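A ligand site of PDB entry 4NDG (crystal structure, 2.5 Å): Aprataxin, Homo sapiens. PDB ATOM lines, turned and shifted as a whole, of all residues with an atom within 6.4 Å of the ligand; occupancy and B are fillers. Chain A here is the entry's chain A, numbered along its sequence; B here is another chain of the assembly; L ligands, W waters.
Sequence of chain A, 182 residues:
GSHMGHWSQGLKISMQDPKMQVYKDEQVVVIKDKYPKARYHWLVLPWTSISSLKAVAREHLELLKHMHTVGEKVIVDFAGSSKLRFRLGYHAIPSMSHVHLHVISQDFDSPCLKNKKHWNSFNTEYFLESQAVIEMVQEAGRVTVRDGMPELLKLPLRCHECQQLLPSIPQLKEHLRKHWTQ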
ATOM      1  N   TRP A   7     -33.514  -1.398  -6.138  1.00  0.00           N
ATOM      2  CA  TRP A   7     -33.461  -2.107  -4.864  1.00  0.00           C
ATOM      3  C   TRP A   7     -32.060  -2.570  -4.529  1.00  0.00           C
ATOM      4  O   TRP A   7     -31.656  -2.558  -3.365  1.00  0.00           O
ATOM      5  CB  TRP A   7     -34.410  -3.314  -4.875  1.00  0.00           C
ATOM      6  CG  TRP A   7     -34.084  -4.315  -5.937  1.00  0.00           C
ATOM      7  CD1 TRP A   7     -34.603  -4.369  -7.202  1.00  0.00           C
ATOM      8  CD2 TRP A   7     -33.183  -5.426  -5.834  1.00  0.00           C
ATOM      9  NE1 TRP A   7     -34.062  -5.427  -7.890  1.00  0.00           N
ATOM     10  CE2 TRP A   7     -33.190  -6.093  -7.067  1.00  0.00           C
ATOM     11  CE3 TRP A   7     -32.369  -5.907  -4.806  1.00  0.00           C
ATOM     12  CZ2 TRP A   7     -32.417  -7.224  -7.306  1.00  0.00           C
ATOM     13  CZ3 TRP A   7     -31.593  -7.019  -5.056  1.00  0.00           C
ATOM     14  CH2 TRP A   7     -31.624  -7.669  -6.292  1.00  0.00           C
ATOM     15  N   GLY A  10     -30.119  -0.281  -2.406  1.00  0.00           N
ATOM     16  CA  GLY A  10     -30.689   0.001  -1.098  1.00  0.00           C
ATOM     17  C   GLY A  10     -29.690   0.320   0.006  1.00  0.00           C
ATOM     18  O   GLY A  10     -29.724   1.415   0.594  1.00  0.00           O
ATOM     19  N   LEU A  11     -28.787  -0.620   0.260  1.00  0.00           N
ATOM     20  CA  LEU A  11     -27.795  -0.475   1.321  1.00  0.00           C
ATOM     21  C   LEU A  11     -27.041   0.850   1.200  1.00  0.00           C
ATOM     22  O   LEU A  11     -26.877   1.572   2.199  1.00  0.00           O
ATOM     23  CB  LEU A  11     -26.789  -1.625   1.267  1.00  0.00           C
ATOM     24  CG  LEU A  11     -27.238  -3.072   1.414  1.00  0.00           C
ATOM     25  CD1 LEU A  11     -26.027  -3.970   1.521  1.00  0.00           C
ATOM     26  CD2 LEU A  11     -28.145  -3.253   2.617  1.00  0.00           C
ATOM     27  N   SER A  14     -28.989   3.557   2.493  1.00  0.00           N
ATOM     28  CA  SER A  14     -29.140   3.443   3.924  1.00  0.00           C
ATOM     29  C   SER A  14     -27.859   3.827   4.642  1.00  0.00           C
ATOM     30  O   SER A  14     -27.920   4.290   5.769  1.00  0.00           O
ATOM     31  CB  SER A  14     -29.578   2.026   4.321  1.00  0.00           C
ATOM     32  OG  SER A  14     -30.940   1.809   3.975  1.00  0.00           O
ATOM     33  N   ILE A  31     -24.869  -0.534  10.020  1.00  0.00           N
ATOM     34  CA  ILE A  31     -26.320  -0.337  10.030  1.00  0.00           C
ATOM     35  C   ILE A  31     -27.073  -1.589  10.427  1.00  0.00           C
ATOM     36  O   ILE A  31     -26.569  -2.702  10.280  1.00  0.00           O
ATOM     37  CB  ILE A  31     -26.856   0.069   8.646  1.00  0.00           C
ATOM     38  CG1 ILE A  31     -26.618  -1.047   7.634  1.00  0.00           C
ATOM     39  CG2 ILE A  31     -26.194   1.352   8.173  1.00  0.00           C
ATOM     40  CD1 ILE A  31     -27.170  -0.767   6.264  1.00  0.00           C
ATOM     41  N   LYS A  32     -28.275  -1.426  10.978  1.00  0.00           N
ATOM     42  CA  LYS A  32     -29.113  -2.577  11.259  1.00  0.00           C
ATOM     43  C   LYS A  32     -29.644  -3.145   9.951  1.00  0.00           C
ATOM     44  O   LYS A  32     -30.052  -2.392   9.069  1.00  0.00           O
ATOM     45  CB  LYS A  32     -30.255  -2.198  12.201  1.00  0.00           C
ATOM     46  CG  LYS A  32     -29.778  -1.698  13.559  1.00  0.00           C
ATOM     47  CD  LYS A  32     -30.759  -1.981  14.684  1.00  0.00           C
ATOM     48  CE  LYS A  32     -32.081  -1.277  14.478  1.00  0.00           C
ATOM     49  NZ  LYS A  32     -32.809  -1.116  15.775  1.00  0.00           N
ATOM     50  N   ASP A  33     -29.636  -4.468   9.823  1.00  0.00           N
ATOM     51  CA  ASP A  33     -30.270  -5.129   8.697  1.00  0.00           C
ATOM     52  C   ASP A  33     -31.751  -4.800   8.713  1.00  0.00           C
ATOM     53  O   ASP A  33     -32.427  -5.001   9.740  1.00  0.00           O
ATOM     54  CB  ASP A  33     -30.074  -6.654   8.760  1.00  0.00           C
ATOM     55  CG  ASP A  33     -30.419  -7.344   7.450  1.00  0.00           C
ATOM     56  OD1 ASP A  33     -31.626  -7.428   7.110  1.00  0.00           O
ATOM     57  OD2 ASP A  33     -29.504  -7.837   6.767  1.00  0.00           O
ATOM     58  N   LYS A  34     -32.266  -4.276   7.609  1.00  0.00           N
ATOM     59  CA  LYS A  34     -33.653  -3.835   7.517  1.00  0.00           C
ATOM     60  C   LYS A  34     -34.657  -4.992   7.632  1.00  0.00           C
ATOM     61  O   LYS A  34     -35.808  -4.785   8.018  1.00  0.00           O
ATOM     62  CB  LYS A  34     -33.877  -3.096   6.199  1.00  0.00           C
ATOM     63  CG  LYS A  34     -35.184  -2.325   6.138  1.00  0.00           C
ATOM     64  CD  LYS A  34     -35.351  -1.633   4.797  1.00  0.00           C
ATOM     65  CE  LYS A  34     -36.644  -0.836   4.766  1.00  0.00           C
ATOM     66  NZ  LYS A  34     -36.849  -0.119   3.479  1.00  0.00           N
ATOM     67  N   TYR A  35     -34.218  -6.193   7.317  1.00  0.00           N
ATOM     68  CA  TYR A  35     -35.050  -7.385   7.432  1.00  0.00           C
ATOM     69  C   TYR A  35     -34.263  -8.450   8.168  1.00  0.00           C
ATOM     70  O   TYR A  35     -33.837  -9.429   7.559  1.00  0.00           O
ATOM     71  CB  TYR A  35     -35.505  -7.891   6.071  1.00  0.00           C
ATOM     72  CG  TYR A  35     -36.099  -6.803   5.215  1.00  0.00           C
ATOM     73  CD1 TYR A  35     -37.433  -6.472   5.333  1.00  0.00           C
ATOM     74  CD2 TYR A  35     -35.318  -6.100   4.295  1.00  0.00           C
ATOM     75  CE1 TYR A  35     -37.991  -5.476   4.553  1.00  0.00           C
ATOM     76  CE2 TYR A  35     -35.861  -5.098   3.520  1.00  0.00           C
ATOM     77  CZ  TYR A  35     -37.202  -4.793   3.654  1.00  0.00           C
ATOM     78  OH  TYR A  35     -37.761  -3.794   2.896  1.00  0.00           O
ATOM     79  N   PRO A  36     -34.042  -8.235   9.466  1.00  0.00           N
ATOM     80  CA  PRO A  36     -33.115  -9.036  10.268  1.00  0.00           C
ATOM     81  C   PRO A  36     -33.512 -10.510  10.336  1.00  0.00           C
ATOM     82  O   PRO A  36     -34.686 -10.837  10.482  1.00  0.00           O
ATOM     83  CB  PRO A  36     -33.203  -8.387  11.652  1.00  0.00           C
ATOM     84  CG  PRO A  36     -34.546  -7.753  11.687  1.00  0.00           C
ATOM     85  CD  PRO A  36     -34.809  -7.279  10.291  1.00  0.00           C
ATOM     86  N   LYS A  37     -32.513 -11.384  10.226  1.00  0.00           N
ATOM     87  CA  LYS A  37     -32.718 -12.831  10.299  1.00  0.00           C
ATOM     88  C   LYS A  37     -32.454 -13.354  11.711  1.00  0.00           C
ATOM     89  O   LYS A  37     -32.297 -14.557  11.923  1.00  0.00           O
ATOM     90  CB  LYS A  37     -31.830 -13.578   9.307  1.00  0.00           C
ATOM     91  CG  LYS A  37     -32.292 -13.591   7.842  1.00  0.00           C
ATOM     92  CD  LYS A  37     -32.533 -12.234   7.229  1.00  0.00           C
ATOM     93  CE  LYS A  37     -33.162 -12.363   5.846  1.00  0.00           C
ATOM     94  NZ  LYS A  37     -33.332 -11.039   5.186  1.00  0.00           N
ATOM     95  N   HIS A  41     -28.854  -8.355  14.151  1.00  0.00           N
ATOM     96  CA  HIS A  41     -28.335  -8.527  12.796  1.00  0.00           C
ATOM     97  C   HIS A  41     -27.881  -7.190  12.229  1.00  0.00           C
ATOM     98  O   HIS A  41     -28.703  -6.317  11.933  1.00  0.00           O
ATOM     99  CB  HIS A  41     -29.411  -9.159  11.906  1.00  0.00           C
ATOM    100  CG  HIS A  41     -28.905  -9.590  10.567  1.00  0.00           C
ATOM    101  ND1 HIS A  41     -29.726 -10.152   9.610  1.00  0.00           N
ATOM    102  CD2 HIS A  41     -27.668  -9.562  10.032  1.00  0.00           C
ATOM    103  CE1 HIS A  41     -29.020 -10.440   8.540  1.00  0.00           C
ATOM    104  NE2 HIS A  41     -27.762 -10.098   8.761  1.00  0.00           N
ATOM    105  N   LEU A  43     -25.106  -5.026   9.471  1.00  0.00           N
ATOM    106  CA  LEU A  43     -24.249  -5.049   8.300  1.00  0.00           C
ATOM    107  C   LEU A  43     -23.124  -4.033   8.464  1.00  0.00           C
ATOM    108  O   LEU A  43     -23.359  -2.869   8.890  1.00  0.00           O
ATOM    109  CB  LEU A  43     -25.061  -4.751   7.032  1.00  0.00           C
ATOM    110  CG  LEU A  43     -26.307  -5.625   6.866  1.00  0.00           C
ATOM    111  CD1 LEU A  43     -27.087  -5.203   5.639  1.00  0.00           C
ATOM    112  CD2 LEU A  43     -25.915  -7.093   6.779  1.00  0.00           C
ATOM    113  N   TYR A  90     -19.537 -13.424   5.264  1.00  0.00           N
ATOM    114  CA  TYR A  90     -20.109 -12.919   4.033  1.00  0.00           C
ATOM    115  C   TYR A  90     -20.876 -13.993   3.285  1.00  0.00           C
ATOM    116  O   TYR A  90     -20.582 -15.175   3.415  1.00  0.00           O
ATOM    117  CB  TYR A  90     -19.000 -12.380   3.109  1.00  0.00           C
ATOM    118  CG  TYR A  90     -18.094 -11.370   3.764  1.00  0.00           C
ATOM    119  CD1 TYR A  90     -16.960 -11.776   4.461  1.00  0.00           C
ATOM    120  CD2 TYR A  90     -18.356 -10.016   3.660  1.00  0.00           C
ATOM    121  CE1 TYR A  90     -16.132 -10.853   5.055  1.00  0.00           C
ATOM    122  CE2 TYR A  90     -17.522  -9.086   4.248  1.00  0.00           C
ATOM    123  CZ  TYR A  90     -16.412  -9.510   4.938  1.00  0.00           C
ATOM    124  OH  TYR A  90     -15.585  -8.591   5.523  1.00  0.00           O
ATOM    125  N   HIS A  91     -21.841 -13.579   2.482  1.00  0.00           N
ATOM    126  CA  HIS A  91     -22.547 -14.487   1.604  1.00  0.00           C
ATOM    127  C   HIS A  91     -21.713 -14.715   0.352  1.00  0.00           C
ATOM    128  O   HIS A  91     -21.141 -13.781  -0.187  1.00  0.00           O
ATOM    129  CB  HIS A  91     -23.916 -13.935   1.224  1.00  0.00           C
ATOM    130  CG  HIS A  91     -24.937 -14.039   2.308  1.00  0.00           C
ATOM    131  ND1 HIS A  91     -26.166 -13.439   2.240  1.00  0.00           N
ATOM    132  CD2 HIS A  91     -24.897 -14.678   3.501  1.00  0.00           C
ATOM    133  CE1 HIS A  91     -26.854 -13.714   3.335  1.00  0.00           C
ATOM    134  NE2 HIS A  91     -26.107 -14.459   4.116  1.00  0.00           N
ATOM    135  N   ILE A  93     -22.697 -15.603  -2.721  1.00  0.00           N
ATOM    136  CA  ILE A  93     -23.300 -14.872  -3.823  1.00  0.00           C
ATOM    137  C   ILE A  93     -24.257 -13.822  -3.295  1.00  0.00           C
ATOM    138  O   ILE A  93     -25.360 -14.138  -2.880  1.00  0.00           O
ATOM    139  CB  ILE A  93     -24.039 -15.823  -4.774  1.00  0.00           C
ATOM    140  CG1 ILE A  93     -23.048 -16.821  -5.375  1.00  0.00           C
ATOM    141  CG2 ILE A  93     -24.759 -15.046  -5.861  1.00  0.00           C
ATOM    142  CD1 ILE A  93     -23.715 -17.921  -6.169  1.00  0.00           C
ATOM    143  N   PRO A  94     -23.844 -12.551  -3.359  1.00  0.00           N
ATOM    144  CA  PRO A  94     -24.693 -11.498  -2.790  1.00  0.00           C
ATOM    145  C   PRO A  94     -25.720 -11.017  -3.788  1.00  0.00           C
ATOM    146  O   PRO A  94     -25.505 -11.085  -4.996  1.00  0.00           O
ATOM    147  CB  PRO A  94     -23.695 -10.390  -2.480  1.00  0.00           C
ATOM    148  CG  PRO A  94     -22.634 -10.553  -3.520  1.00  0.00           C
ATOM    149  CD  PRO A  94     -22.565 -12.021  -3.854  1.00  0.00           C
ATOM    150  N   SER A  95     -26.861 -10.565  -3.283  1.00  0.00           N
ATOM    151  CA  SER A  95     -27.907 -10.030  -4.131  1.00  0.00           C
ATOM    152  C   SER A  95     -27.754  -8.519  -4.215  1.00  0.00           C
ATOM    153  O   SER A  95     -27.914  -7.920  -5.275  1.00  0.00           O
ATOM    154  CB  SER A  95     -29.297 -10.395  -3.594  1.00  0.00           C
ATOM    155  OG  SER A  95     -29.363 -11.772  -3.278  1.00  0.00           O
ATOM    156  N   MET A  96     -27.469  -7.895  -3.076  1.00  0.00           N
ATOM    157  CA  MET A  96     -27.280  -6.449  -3.029  1.00  0.00           C
ATOM    158  C   MET A  96     -25.880  -6.050  -3.471  1.00  0.00           C
ATOM    159  O   MET A  96     -24.910  -6.748  -3.179  1.00  0.00           O
ATOM    160  CB  MET A  96     -27.538  -5.929  -1.603  1.00  0.00           C
ATOM    161  CG  MET A  96     -28.896  -6.315  -1.039  1.00  0.00           C
ATOM    162  SD  MET A  96     -30.227  -5.263  -1.644  1.00  0.00           S
ATOM    163  CE  MET A  96     -30.156  -3.908  -0.478  1.00  0.00           C
ATOM    164  N   SER A  97     -25.783  -4.883  -4.111  1.00  0.00           N
ATOM    165  CA  SER A  97     -24.490  -4.348  -4.507  1.00  0.00           C
ATOM    166  C   SER A  97     -23.808  -3.807  -3.270  1.00  0.00           C
ATOM    167  O   SER A  97     -24.478  -3.582  -2.244  1.00  0.00           O
ATOM    168  CB  SER A  97     -24.636  -3.256  -5.548  1.00  0.00           C
ATOM    169  OG  SER A  97     -25.322  -3.716  -6.700  1.00  0.00           O
ATOM    170  N   HIS A  98     -22.484  -3.669  -3.328  1.00  0.00           N
ATOM    171  CA  HIS A  98     -21.658  -3.111  -2.252  1.00  0.00           C
ATOM    172  C   HIS A  98     -21.444  -4.214  -1.211  1.00  0.00           C
ATOM    173  O   HIS A  98     -22.404  -4.729  -0.630  1.00  0.00           O
ATOM    174  CB  HIS A  98     -22.327  -1.879  -1.628  1.00  0.00           C
ATOM    175  CG  HIS A  98     -21.378  -0.917  -0.992  1.00  0.00           C
ATOM    176  ND1 HIS A  98     -20.551  -1.233   0.072  1.00  0.00           N
ATOM    177  CD2 HIS A  98     -21.156   0.397  -1.242  1.00  0.00           C
ATOM    178  CE1 HIS A  98     -19.844  -0.167   0.408  1.00  0.00           C
ATOM    179  NE2 HIS A  98     -20.202   0.835  -0.367  1.00  0.00           N
ATOM    180  N   HIS A 100     -20.783  -6.398   2.063  1.00  0.00           N
ATOM    181  CA  HIS A 100     -21.301  -6.195   3.401  1.00  0.00           C
ATOM    182  C   HIS A 100     -21.007  -7.382   4.317  1.00  0.00           C
ATOM    183  O   HIS A 100     -21.255  -8.536   3.960  1.00  0.00           O
ATOM    184  CB  HIS A 100     -22.812  -5.897   3.383  1.00  0.00           C
ATOM    185  CG  HIS A 100     -23.601  -6.731   2.415  1.00  0.00           C
ATOM    186  ND1 HIS A 100     -23.637  -6.466   1.064  1.00  0.00           N
ATOM    187  CD2 HIS A 100     -24.431  -7.779   2.625  1.00  0.00           C
ATOM    188  CE1 HIS A 100     -24.441  -7.335   0.469  1.00  0.00           C
ATOM    189  NE2 HIS A 100     -24.940  -8.146   1.390  1.00  0.00           N
ATOM    190  N   HIS A 102     -21.883  -9.552   7.384  1.00  0.00           N
ATOM    191  CA  HIS A 102     -22.992  -9.908   8.255  1.00  0.00           C
ATOM    192  C   HIS A 102     -22.469 -10.154   9.659  1.00  0.00           C
ATOM    193  O   HIS A 102     -21.541 -10.946   9.861  1.00  0.00           O
ATOM    194  CB  HIS A 102     -23.720 -11.144   7.749  1.00  0.00           C
ATOM    195  CG  HIS A 102     -24.532 -10.909   6.515  1.00  0.00           C
ATOM    196  ND1 HIS A 102     -25.838 -10.449   6.556  1.00  0.00           N
ATOM    197  CD2 HIS A 102     -24.237 -11.076   5.202  1.00  0.00           C
ATOM    198  CE1 HIS A 102     -26.294 -10.336   5.324  1.00  0.00           C
ATOM    199  NE2 HIS A 102     -25.345 -10.707   4.483  1.00  0.00           N
ATOM    200  N   PHE A 122     -27.413 -18.705   5.919  1.00  0.00           N
ATOM    201  CA  PHE A 122     -26.609 -18.486   7.115  1.00  0.00           C
ATOM    202  C   PHE A 122     -26.030 -19.756   7.771  1.00  0.00           C
ATOM    203  O   PHE A 122     -25.189 -19.649   8.658  1.00  0.00           O
ATOM    204  CB  PHE A 122     -27.416 -17.705   8.139  1.00  0.00           C
ATOM    205  CG  PHE A 122     -27.567 -16.260   7.782  1.00  0.00           C
ATOM    206  CD1 PHE A 122     -26.522 -15.371   7.967  1.00  0.00           C
ATOM    207  CD2 PHE A 122     -28.738 -15.793   7.224  1.00  0.00           C
ATOM    208  CE1 PHE A 122     -26.666 -14.034   7.631  1.00  0.00           C
ATOM    209  CE2 PHE A 122     -28.891 -14.471   6.876  1.00  0.00           C
ATOM    210  CZ  PHE A 122     -27.850 -13.585   7.075  1.00  0.00           C
ATOM    211  OP3   G B   1     -27.518 -11.379   1.310  1.00  0.00           O
ATOM    212  P     G B   1     -28.735 -11.807   0.343  1.00  0.00           P
ATOM    213  OP1   G B   1     -29.418 -12.833   1.136  1.00  0.00           O
ATOM    214  OP2   G B   1     -28.278 -12.204  -1.002  1.00  0.00           O
ATOM    215  O5'   G B   1     -29.736 -10.593   0.151  1.00  0.00           O
ATOM    216  C5'   G B   1     -31.129 -10.819   0.076  1.00  0.00           C
ATOM    217  C4'   G B   1     -31.898  -9.519   0.069  1.00  0.00           C
ATOM    218  O4'   G B   1     -31.749  -8.856  -1.207  1.00  0.00           O
ATOM    219  C3'   G B   1     -33.398  -9.660   0.231  1.00  0.00           C
ATOM    220  O3'   G B   1     -33.761  -9.810   1.583  1.00  0.00           O
ATOM    221  C2'   G B   1     -33.929  -8.390  -0.414  1.00  0.00           C
ATOM    222  O2'   G B   1     -33.816  -7.288   0.483  1.00  0.00           O
ATOM    223  C1'   G B   1     -32.931  -8.170  -1.544  1.00  0.00           C
ATOM    224  N9    G B   1     -33.405  -8.641  -2.860  1.00  0.00           N
ATOM    225  C8    G B   1     -32.872  -9.669  -3.598  1.00  0.00           C
ATOM    226  N7    G B   1     -33.452  -9.841  -4.748  1.00  0.00           N
ATOM    227  C5    G B   1     -34.420  -8.863  -4.784  1.00  0.00           C
ATOM    228  C6    G B   1     -35.362  -8.560  -5.788  1.00  0.00           C
ATOM    229  O6    G B   1     -35.534  -9.118  -6.876  1.00  0.00           O
ATOM    230  N1    G B   1     -36.178  -7.482  -5.428  1.00  0.00           N
ATOM    231  C2    G B   1     -36.085  -6.793  -4.252  1.00  0.00           C
ATOM    232  N2    G B   1     -36.962  -5.787  -4.093  1.00  0.00           N
ATOM    233  N3    G B   1     -35.206  -7.056  -3.301  1.00  0.00           N
ATOM    234  C4    G B   1     -34.412  -8.105  -3.626  1.00  0.00           C
ATOM    235  P    DT B   2     -35.015 -10.727   1.968  1.00  0.00           P
ATOM    236  OP1  DT B   2     -35.003 -10.881   3.440  1.00  0.00           O
ATOM    237  OP2  DT B   2     -34.978 -11.937   1.128  1.00  0.00           O
ATOM    238  O5'  DT B   2     -36.270  -9.855   1.502  1.00  0.00           O
ATOM    239  C5'  DT B   2     -36.590  -8.636   2.128  1.00  0.00           C
ATOM    240  C4'  DT B   2     -37.727  -8.000   1.376  1.00  0.00           C
ATOM    241  O4'  DT B   2     -37.361  -7.961  -0.022  1.00  0.00           O
ATOM    242  C3'  DT B   2     -39.042  -8.773   1.429  1.00  0.00           C
ATOM    243  O3'  DT B   2     -39.959  -8.111   2.277  1.00  0.00           O
ATOM    244  C2'  DT B   2     -39.589  -8.738   0.017  1.00  0.00           C
ATOM    245  C1'  DT B   2     -38.501  -8.110  -0.834  1.00  0.00           C
ATOM    246  N1   DT B   2     -38.154  -8.943  -2.005  1.00  0.00           N
ATOM    247  C2   DT B   2     -38.817  -8.677  -3.176  1.00  0.00           C
ATOM    248  O2   DT B   2     -39.637  -7.784  -3.285  1.00  0.00           O
ATOM    249  N3   DT B   2     -38.449  -9.475  -4.221  1.00  0.00           N
ATOM    250  C4   DT B   2     -37.530 -10.508  -4.212  1.00  0.00           C
ATOM    251  O4   DT B   2     -37.291 -11.151  -5.227  1.00  0.00           O
ATOM    252  C5   DT B   2     -36.889 -10.750  -2.932  1.00  0.00           C
ATOM    253  C7   DT B   2     -35.879 -11.833  -2.755  1.00  0.00           C
ATOM    254  C6   DT B   2     -37.236  -9.961  -1.899  1.00  0.00           C
HETATM  255  O1  LIG L   1     -25.180 -10.784   1.425  1.00  0.00           O
HETATM  256  V1  LIG L   1     -26.335  -9.746   1.169  1.00  0.00           V
HETATM  257  O2  LIG L   1     -26.709  -9.319  -0.291  1.00  0.00           O
HETATM  258  O3  LIG L   1     -27.071  -9.052   2.491  1.00  0.00           O
HETATM  259  C1  LIG L   1     -28.270  -8.352   2.174  1.00  0.00           C
HETATM  260  C2  LIG L   1     -29.022  -8.005   3.434  1.00  0.00           C
HETATM  261  C3  LIG L   1     -30.334  -8.770   3.680  1.00  0.00           C
HETATM  262  O4  LIG L   1     -30.292  -9.370   4.968  1.00  0.00           O
HETATM  263  C4  LIG L   1     -31.417  -7.693   3.653  1.00  0.00           C
HETATM  264  O5  LIG L   1     -32.482  -7.912   4.554  1.00  0.00           O
HETATM  265  C5  LIG L   1     -30.636  -6.429   4.014  1.00  0.00           C
HETATM  266  O6  LIG L   1     -29.370  -6.598   3.427  1.00  0.00           O
HETATM  267  N1  LIG L   1     -31.192  -5.196   3.454  1.00  0.00           N
HETATM  268  C6  LIG L   1     -31.081  -3.924   3.978  1.00  0.00           C
HETATM  269  C7  LIG L   1     -31.737  -3.072   3.080  1.00  0.00           C
HETATM  270  N2  LIG L   1     -32.218  -3.844   2.070  1.00  0.00           N
HETATM  271  C8  LIG L   1     -31.889  -5.082   2.282  1.00  0.00           C
HETATM  272  N3  LIG L   1     -30.515  -3.400   5.067  1.00  0.00           N
HETATM  273  C9  LIG L   1     -30.578  -2.100   5.304  1.00  0.00           C
HETATM  274  N4  LIG L   1     -31.194  -1.264   4.486  1.00  0.00           N
HETATM  275  C10 LIG L   1     -31.781  -1.698   3.377  1.00  0.00           C
HETATM  276  N5  LIG L   1     -32.424  -0.817   2.530  1.00  0.00           N
HETATM  277  O   HOH W   1     -22.479 -10.601   2.154  1.00  0.00           O
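The backbone NH of Lys 34 lies within hydrogen-bond range of a nitrogen (N3) of the ligand, 3.2 Å away.
OP3 of G 1 of chain B is bound to V1 of the ligand, 2.0 Å away.
A ring nitrogen (NE2) of His 100 binds a vanadium atom (V1) of the ligand.
An oxygen (O5) of the ligand is in hydrogen-bond range of the side-chain amino group (NZ) of Lys 37, at 3.3 Å.
The side-chain hydroxyl of Ser 14 is in hydrogen-bond range of a nitrogen (N4) of the ligand.
OD2 of Asp 33 lies within hydrogen-bond range of O4 of the ligand, at 2.5 Å.
OP1 of G 1 of chain B lies within hydrogen-bond range of a ring nitrogen (ND1) of His 91.
The side-chain amino group (NZ) of Lys 37 is in salt-bridge range of OP1 of DT 2 of chain B (2.4 Å).
N of Lys 37 sits at hydrogen-bond distance from ND1 of His 41 (3.1 Å).
O of Tyr 35 is in hydrogen-bond range of NZ of Lys 37 (2.9 Å).
N of Leu 43 sits at hydrogen-bond distance from O of Ile 31 (2.9 Å).
OP2 of G 1 of chain B sits at hydrogen-bond distance from OG of Ser 95 (2.6 Å).
ND1 of His 102 sits at hydrogen-bond distance from NE2 of His 41 (2.9 Å).
The backbone NH (N) of Asp 33 is in hydrogen-bond range of the backbone carbonyl oxygen (O) of His 41, at 3.0 Å.
A ring nitrogen (ND1) of His 91 lies close to an oxygen (O1) of the ligand, 2.9 Å away.
The backbone NH (N) of Ser 95 sits close to an oxygen (O2) of the ligand, 3.2 Å away.
N of Met 96 lies close to O2 of the ligand (3.2 Å).
A ring nitrogen (NE2) of His 102 lies close to an oxygen (O1) of the ligand (3.1 Å).
Residues that only touch the ligand: Gly 10 (3.9 Å), Leu 11 (3.3 Å), Ile 31 (3.8 Å), Lys 32 (3.8 Å), Tyr 35 (3.4 Å), His 41 (3.9 Å), Leu 43 (3.5 Å) and Pro 94 (3.9 Å).
Hydrophobic or aromatic side chains that line the ligand: Leu 11, Ile 31, Tyr 35, His 41, Leu 43, His 91, Pro 94, Met 96, His 100 and His 102.
18 residues have an atom within 4 Å of the ligand: Gly 10, Leu 11, Ser 14, Ile 31, Lys 32, Asp 33, Lys 34, Tyr 35, Lys 37, His 41, Leu 43, His 91, Pro 94, Ser 95, Met 96, His 100, His 102 and G 1 of chain B.
The nearest printed residue that does not touch the ligand is DT 2 of chain B (4.1 Å).
Water W1 lies within hydrogen-bond range of the backbone carbonyl oxygen (O) of His 100 (3.0 Å) and the backbone NH (N) of His 91 (3.1 Å).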
